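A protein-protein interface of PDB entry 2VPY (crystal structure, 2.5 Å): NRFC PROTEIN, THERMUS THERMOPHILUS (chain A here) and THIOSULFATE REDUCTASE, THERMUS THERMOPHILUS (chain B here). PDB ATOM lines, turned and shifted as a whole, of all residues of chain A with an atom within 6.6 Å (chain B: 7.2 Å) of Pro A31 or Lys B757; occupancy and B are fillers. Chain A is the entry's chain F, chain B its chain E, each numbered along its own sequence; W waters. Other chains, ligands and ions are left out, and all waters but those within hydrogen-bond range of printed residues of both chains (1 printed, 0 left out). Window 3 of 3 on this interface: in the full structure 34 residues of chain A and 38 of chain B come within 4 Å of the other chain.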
ATOM      1  N   LYS A  24     -38.288 -17.970 -11.188  1.00  0.00           N
ATOM      2  CA  LYS A  24     -37.550 -17.345 -12.315  1.00  0.00           C
ATOM      3  C   LYS A  24     -38.261 -17.350 -13.669  1.00  0.00           C
ATOM      4  O   LYS A  24     -38.014 -16.500 -14.528  1.00  0.00           O
ATOM      5  CB  LYS A  24     -36.242 -18.077 -12.577  1.00  0.00           C
ATOM      6  CG  LYS A  24     -35.067 -17.569 -11.862  1.00  0.00           C
ATOM      7  CD  LYS A  24     -34.374 -16.499 -12.637  1.00  0.00           C
ATOM      8  CE  LYS A  24     -33.201 -16.078 -11.807  1.00  0.00           C
ATOM      9  NZ  LYS A  24     -32.384 -15.038 -12.452  1.00  0.00           N
ATOM     10  N   VAL A  29     -37.684 -13.253 -13.585  1.00  0.00           N
ATOM     11  CA  VAL A  29     -36.642 -12.612 -12.793  1.00  0.00           C
ATOM     12  C   VAL A  29     -35.389 -12.721 -13.696  1.00  0.00           C
ATOM     13  O   VAL A  29     -35.078 -13.787 -14.221  1.00  0.00           O
ATOM     14  CB  VAL A  29     -36.498 -13.324 -11.389  1.00  0.00           C
ATOM     15  CG1 VAL A  29     -35.512 -12.571 -10.498  1.00  0.00           C
ATOM     16  CG2 VAL A  29     -37.889 -13.388 -10.713  1.00  0.00           C
ATOM     17  N   PRO A  30     -34.690 -11.592 -13.917  1.00  0.00           N
ATOM     18  CA  PRO A  30     -33.482 -11.395 -14.739  1.00  0.00           C
ATOM     19  C   PRO A  30     -32.236 -12.157 -14.257  1.00  0.00           C
ATOM     20  O   PRO A  30     -32.175 -12.517 -13.088  1.00  0.00           O
ATOM     21  CB  PRO A  30     -33.257  -9.876 -14.675  1.00  0.00           C
ATOM     22  CG  PRO A  30     -34.492  -9.314 -13.895  1.00  0.00           C
ATOM     23  CD  PRO A  30     -34.863 -10.448 -13.014  1.00  0.00           C
ATOM     24  N   PRO A  31     -31.249 -12.435 -15.157  1.00  0.00           N
ATOM     25  CA  PRO A  31     -30.019 -13.148 -14.759  1.00  0.00           C
ATOM     26  C   PRO A  31     -29.228 -12.419 -13.650  1.00  0.00           C
ATOM     27  O   PRO A  31     -29.108 -11.195 -13.679  1.00  0.00           O
ATOM     28  CB  PRO A  31     -29.162 -13.159 -16.024  1.00  0.00           C
ATOM     29  CG  PRO A  31     -30.114 -13.090 -17.151  1.00  0.00           C
ATOM     30  CD  PRO A  31     -31.405 -12.454 -16.627  1.00  0.00           C
ATOM     31  N   GLY A  32     -28.661 -13.165 -12.704  1.00  0.00           N
ATOM     32  CA  GLY A  32     -27.860 -12.572 -11.650  1.00  0.00           C
ATOM     33  C   GLY A  32     -28.572 -12.209 -10.367  1.00  0.00           C
ATOM     34  O   GLY A  32     -27.924 -11.900  -9.372  1.00  0.00           O
ATOM     35  N   VAL A  33     -29.898 -12.239 -10.382  1.00  0.00           N
ATOM     36  CA  VAL A  33     -30.657 -11.917  -9.195  1.00  0.00           C
ATOM     37  C   VAL A  33     -31.756 -12.950  -8.970  1.00  0.00           C
ATOM     38  O   VAL A  33     -32.245 -13.578  -9.917  1.00  0.00           O
ATOM     39  CB  VAL A  33     -31.149 -10.467  -9.277  1.00  0.00           C
ATOM     40  CG1 VAL A  33     -29.927  -9.540  -9.350  1.00  0.00           C
ATOM     41  CG2 VAL A  33     -32.019 -10.274 -10.502  1.00  0.00           C
ATOM     42  N   PHE A  34     -32.134 -13.110  -7.711  1.00  0.00           N
ATOM     43  CA  PHE A  34     -33.056 -14.162  -7.320  1.00  0.00           C
ATOM     44  C   PHE A  34     -34.132 -13.775  -6.312  1.00  0.00           C
ATOM     45  O   PHE A  34     -33.821 -13.173  -5.300  1.00  0.00           O
ATOM     46  CB  PHE A  34     -32.196 -15.303  -6.703  1.00  0.00           C
ATOM     47  CG  PHE A  34     -31.124 -15.863  -7.627  1.00  0.00           C
ATOM     48  CD1 PHE A  34     -29.839 -15.291  -7.712  1.00  0.00           C
ATOM     49  CD2 PHE A  34     -31.425 -16.939  -8.453  1.00  0.00           C
ATOM     50  CE1 PHE A  34     -28.880 -15.789  -8.621  1.00  0.00           C
ATOM     51  CE2 PHE A  34     -30.485 -17.451  -9.358  1.00  0.00           C
ATOM     52  CZ  PHE A  34     -29.213 -16.877  -9.451  1.00  0.00           C
ATOM     53  N   PRO A 109     -32.531  -4.583 -13.149  1.00  0.00           N
ATOM     54  CA  PRO A 109     -31.802  -3.860 -14.205  1.00  0.00           C
ATOM     55  C   PRO A 109     -32.636  -2.769 -14.903  1.00  0.00           C
ATOM     56  O   PRO A 109     -32.130  -2.031 -15.754  1.00  0.00           O
ATOM     57  CB  PRO A 109     -31.342  -4.958 -15.172  1.00  0.00           C
ATOM     58  CG  PRO A 109     -32.046  -6.221 -14.714  1.00  0.00           C
ATOM     59  CD  PRO A 109     -32.286  -6.026 -13.243  1.00  0.00           C
ATOM     60  N   PRO B  92     -29.236 -18.568 -27.514  1.00  0.00           N
ATOM     61  CA  PRO B  92     -28.674 -18.067 -28.775  1.00  0.00           C
ATOM     62  C   PRO B  92     -27.958 -19.399 -29.169  1.00  0.00           C
ATOM     63  O   PRO B  92     -28.639 -20.338 -29.542  1.00  0.00           O
ATOM     64  CB  PRO B  92     -27.714 -16.957 -28.317  1.00  0.00           C
ATOM     65  CG  PRO B  92     -28.448 -16.350 -27.129  1.00  0.00           C
ATOM     66  CD  PRO B  92     -29.091 -17.572 -26.431  1.00  0.00           C
ATOM     67  N   TRP B 638     -28.948 -20.954 -19.265  1.00  0.00           N
ATOM     68  CA  TRP B 638     -28.616 -19.934 -18.255  1.00  0.00           C
ATOM     69  C   TRP B 638     -29.483 -20.007 -17.008  1.00  0.00           C
ATOM     70  O   TRP B 638     -28.998 -19.819 -15.895  1.00  0.00           O
ATOM     71  CB  TRP B 638     -28.594 -18.465 -18.815  1.00  0.00           C
ATOM     72  CG  TRP B 638     -29.923 -17.749 -19.109  1.00  0.00           C
ATOM     73  CD1 TRP B 638     -30.510 -17.622 -20.333  1.00  0.00           C
ATOM     74  CD2 TRP B 638     -30.813 -17.088 -18.163  1.00  0.00           C
ATOM     75  NE1 TRP B 638     -31.702 -16.935 -20.220  1.00  0.00           N
ATOM     76  CE2 TRP B 638     -31.916 -16.592 -18.912  1.00  0.00           C
ATOM     77  CE3 TRP B 638     -30.785 -16.863 -16.774  1.00  0.00           C
ATOM     78  CZ2 TRP B 638     -32.987 -15.902 -18.320  1.00  0.00           C
ATOM     79  CZ3 TRP B 638     -31.876 -16.163 -16.175  1.00  0.00           C
ATOM     80  CH2 TRP B 638     -32.949 -15.695 -16.958  1.00  0.00           C
ATOM     81  N   GLU B 642     -27.244 -20.901 -13.653  1.00  0.00           N
ATOM     82  CA  GLU B 642     -27.288 -19.847 -12.639  1.00  0.00           C
ATOM     83  C   GLU B 642     -27.515 -20.472 -11.254  1.00  0.00           C
ATOM     84  O   GLU B 642     -27.048 -19.951 -10.231  1.00  0.00           O
ATOM     85  CB  GLU B 642     -28.413 -18.893 -12.972  1.00  0.00           C
ATOM     86  CG  GLU B 642     -28.068 -17.455 -12.843  1.00  0.00           C
ATOM     87  CD  GLU B 642     -29.275 -16.571 -12.982  1.00  0.00           C
ATOM     88  OE1 GLU B 642     -30.383 -17.119 -13.108  1.00  0.00           O
ATOM     89  OE2 GLU B 642     -29.104 -15.343 -12.959  1.00  0.00           O
ATOM     90  N   LEU B 708     -21.760 -20.863 -22.549  1.00  0.00           N
ATOM     91  CA  LEU B 708     -21.870 -20.966 -21.091  1.00  0.00           C
ATOM     92  C   LEU B 708     -21.246 -22.276 -20.577  1.00  0.00           C
ATOM     93  O   LEU B 708     -20.552 -22.295 -19.571  1.00  0.00           O
ATOM     94  CB  LEU B 708     -23.331 -21.008 -20.621  1.00  0.00           C
ATOM     95  CG  LEU B 708     -24.513 -20.086 -20.953  1.00  0.00           C
ATOM     96  CD1 LEU B 708     -25.022 -19.561 -19.617  1.00  0.00           C
ATOM     97  CD2 LEU B 708     -24.170 -18.941 -21.913  1.00  0.00           C
ATOM     98  N   LEU B 752     -20.876 -15.389 -16.375  1.00  0.00           N
ATOM     99  CA  LEU B 752     -22.024 -16.165 -16.749  1.00  0.00           C
ATOM    100  C   LEU B 752     -23.298 -15.301 -16.871  1.00  0.00           C
ATOM    101  O   LEU B 752     -24.174 -15.573 -17.692  1.00  0.00           O
ATOM    102  CB  LEU B 752     -22.147 -17.238 -15.695  1.00  0.00           C
ATOM    103  CG  LEU B 752     -22.621 -18.564 -16.167  1.00  0.00           C
ATOM    104  CD1 LEU B 752     -21.974 -19.637 -15.332  1.00  0.00           C
ATOM    105  CD2 LEU B 752     -24.118 -18.584 -16.061  1.00  0.00           C
ATOM    106  N   THR B 753     -23.396 -14.256 -16.059  1.00  0.00           N
ATOM    107  CA  THR B 753     -24.562 -13.375 -16.114  1.00  0.00           C
ATOM    108  C   THR B 753     -24.492 -12.583 -17.421  1.00  0.00           C
ATOM    109  O   THR B 753     -25.501 -12.386 -18.103  1.00  0.00           O
ATOM    110  CB  THR B 753     -24.623 -12.372 -14.905  1.00  0.00           C
ATOM    111  OG1 THR B 753     -24.545 -13.090 -13.675  1.00  0.00           O
ATOM    112  CG2 THR B 753     -25.945 -11.562 -14.937  1.00  0.00           C
ATOM    113  N   GLY B 754     -23.281 -12.142 -17.748  1.00  0.00           N
ATOM    114  CA  GLY B 754     -23.013 -11.409 -18.973  1.00  0.00           C
ATOM    115  C   GLY B 754     -23.397 -12.255 -20.173  1.00  0.00           C
ATOM    116  O   GLY B 754     -24.003 -11.776 -21.134  1.00  0.00           O
ATOM    117  N   LEU B 755     -23.036 -13.528 -20.132  1.00  0.00           N
ATOM    118  CA  LEU B 755     -23.437 -14.425 -21.198  1.00  0.00           C
ATOM    119  C   LEU B 755     -24.958 -14.697 -21.105  1.00  0.00           C
ATOM    120  O   LEU B 755     -25.619 -14.793 -22.136  1.00  0.00           O
ATOM    121  CB  LEU B 755     -22.637 -15.744 -21.144  1.00  0.00           C
ATOM    122  CG  LEU B 755     -21.198 -15.637 -21.687  1.00  0.00           C
ATOM    123  CD1 LEU B 755     -20.302 -16.761 -21.181  1.00  0.00           C
ATOM    124  CD2 LEU B 755     -21.236 -15.649 -23.206  1.00  0.00           C
ATOM    125  N   ALA B 756     -25.539 -14.782 -19.909  1.00  0.00           N
ATOM    126  CA  ALA B 756     -26.977 -15.068 -19.843  1.00  0.00           C
ATOM    127  C   ALA B 756     -27.863 -13.988 -20.458  1.00  0.00           C
ATOM    128  O   ALA B 756     -28.965 -14.265 -20.936  1.00  0.00           O
ATOM    129  CB  ALA B 756     -27.425 -15.328 -18.383  1.00  0.00           C
ATOM    130  N   LYS B 757     -27.347 -12.767 -20.466  1.00  0.00           N
ATOM    131  CA  LYS B 757     -28.066 -11.595 -20.952  1.00  0.00           C
ATOM    132  C   LYS B 757     -28.222 -11.360 -22.450  1.00  0.00           C
ATOM    133  O   LYS B 757     -29.131 -10.626 -22.869  1.00  0.00           O
ATOM    134  CB  LYS B 757     -27.505 -10.364 -20.257  1.00  0.00           C
ATOM    135  CG  LYS B 757     -27.997 -10.289 -18.834  1.00  0.00           C
ATOM    136  CD  LYS B 757     -27.257  -9.264 -18.026  1.00  0.00           C
ATOM    137  CE  LYS B 757     -27.899  -9.143 -16.655  1.00  0.00           C
ATOM    138  NZ  LYS B 757     -27.603  -7.851 -15.981  1.00  0.00           N
ATOM    139  N   ARG B 758     -27.332 -11.961 -23.241  1.00  0.00           N
ATOM    140  CA  ARG B 758     -27.426 -11.913 -24.697  1.00  0.00           C
ATOM    141  C   ARG B 758     -28.864 -12.239 -24.976  1.00  0.00           C
ATOM    142  O   ARG B 758     -29.350 -13.287 -24.558  1.00  0.00           O
ATOM    143  CB  ARG B 758     -26.633 -13.021 -25.350  1.00  0.00           C
ATOM    144  CG  ARG B 758     -25.185 -12.849 -25.265  1.00  0.00           C
ATOM    145  CD  ARG B 758     -24.581 -14.116 -24.748  1.00  0.00           C
ATOM    146  NE  ARG B 758     -24.179 -15.028 -25.813  1.00  0.00           N
ATOM    147  CZ  ARG B 758     -24.471 -16.323 -25.855  1.00  0.00           C
ATOM    148  NH1 ARG B 758     -25.191 -16.883 -24.889  1.00  0.00           N
ATOM    149  NH2 ARG B 758     -24.010 -17.065 -26.850  1.00  0.00           N
ATOM    150  N   PRO B 759     -29.557 -11.365 -25.710  1.00  0.00           N
ATOM    151  CA  PRO B 759     -30.964 -11.582 -26.037  1.00  0.00           C
ATOM    152  C   PRO B 759     -31.149 -12.645 -27.106  1.00  0.00           C
ATOM    153  O   PRO B 759     -30.284 -12.852 -27.967  1.00  0.00           O
ATOM    154  CB  PRO B 759     -31.452 -10.204 -26.509  1.00  0.00           C
ATOM    155  CG  PRO B 759     -30.257  -9.257 -26.311  1.00  0.00           C
ATOM    156  CD  PRO B 759     -29.050 -10.139 -26.336  1.00  0.00           C
ATOM    157  N   PHE B 760     -32.285 -13.324 -27.033  1.00  0.00           N
ATOM    158  CA  PHE B 760     -32.613 -14.336 -28.003  1.00  0.00           C
ATOM    159  C   PHE B 760     -33.274 -13.708 -29.213  1.00  0.00           C
ATOM    160  O   PHE B 760     -34.405 -13.202 -29.162  1.00  0.00           O
ATOM    161  CB  PHE B 760     -33.545 -15.398 -27.443  1.00  0.00           C
ATOM    162  CG  PHE B 760     -33.869 -16.453 -28.443  1.00  0.00           C
ATOM    163  CD1 PHE B 760     -32.851 -17.240 -28.976  1.00  0.00           C
ATOM    164  CD2 PHE B 760     -35.172 -16.645 -28.881  1.00  0.00           C
ATOM    165  CE1 PHE B 760     -33.120 -18.194 -29.936  1.00  0.00           C
ATOM    166  CE2 PHE B 760     -35.457 -17.599 -29.849  1.00  0.00           C
ATOM    167  CZ  PHE B 760     -34.427 -18.380 -30.376  1.00  0.00           C
HETATM  168  O   HOH W   1     -30.157  -8.577 -14.029  1.00  0.00           O
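NZ of Lys A24 is in salt-bridge range of OE1 of Glu B642 (3.0 Å). The side-chain carboxylate (OE2) of Glu B642 lies close to the backbone NH (N) of Gly A32 (2.2 Å).
O of Lys A24 lies within hydrogen-bond range of N of Val A29 (3.4 Å). The side-chain amino group (NZ) of Lys A24 lies within hydrogen-bond range of the backbone carbonyl oxygen (O) of Pro A30, 2.6 Å away. The backbone carbonyl oxygen (O) of Val A33 is in hydrogen-bond range of the side-chain amino group (NZ) of Lys A24, at 2.9 Å.
Among the printed residues, merely in contact across the chains: Pro A31 with Glu B642, Pro A31 with Thr B753, Phe A34 with Glu B642, Pro A31 with Trp B638, Pro A31 with Ala B756, Pro A31 with Lys B757, Gly A32 with Thr B753, Lys A24 with Trp B638 and Val A29 with Trp B638.
Printed residues of chain A within 4 Å of Trp B638: Lys A24, Val A29 and Pro A31. Printed residues of chain A within 4 Å of Thr B753: Pro A31 and Gly A32. Of the printed residues of chain B, Val A29 touches Trp B638 (3.96 Å). Of the printed residues of chain B, Gly A32 touches Glu B642 and Thr B753. Of the printed residues of chain B, Lys A24 touches Trp B638 (3.9 Å) and Glu B642 (3.0 Å). Gly B754 touches none of the printed residues of chain A. Pro B759 touches none of the printed residues of chain A. The nearest residue of chain B that does not touch Pro A31 is Leu B752 (5.8 Å). The nearest printed residue of chain A that does not touch Ala B756 is Gly A32 (6.2 Å).
Of the 13 printed residues of chain B, 5 touch a printed residue of chain A. Printed residues of chain A that touch a printed residue of chain B: Lys A24, Val A29, Pro A31, Gly A32 and Phe A34. Along chain A the printed residues that touch a printed residue of chain B span positions 24 to 34. Among the printed residues, Asp or Glu carboxylates within 4 Å of a Lys or Arg side-chain nitrogen of the other chain: Lys A24 with Glu B642.
Water W1 bridges the backbone carbonyl oxygen (O) of Pro A31 (2.8 Å) and the side-chain amino group (NZ) of Lys B757 (3.3 Å).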
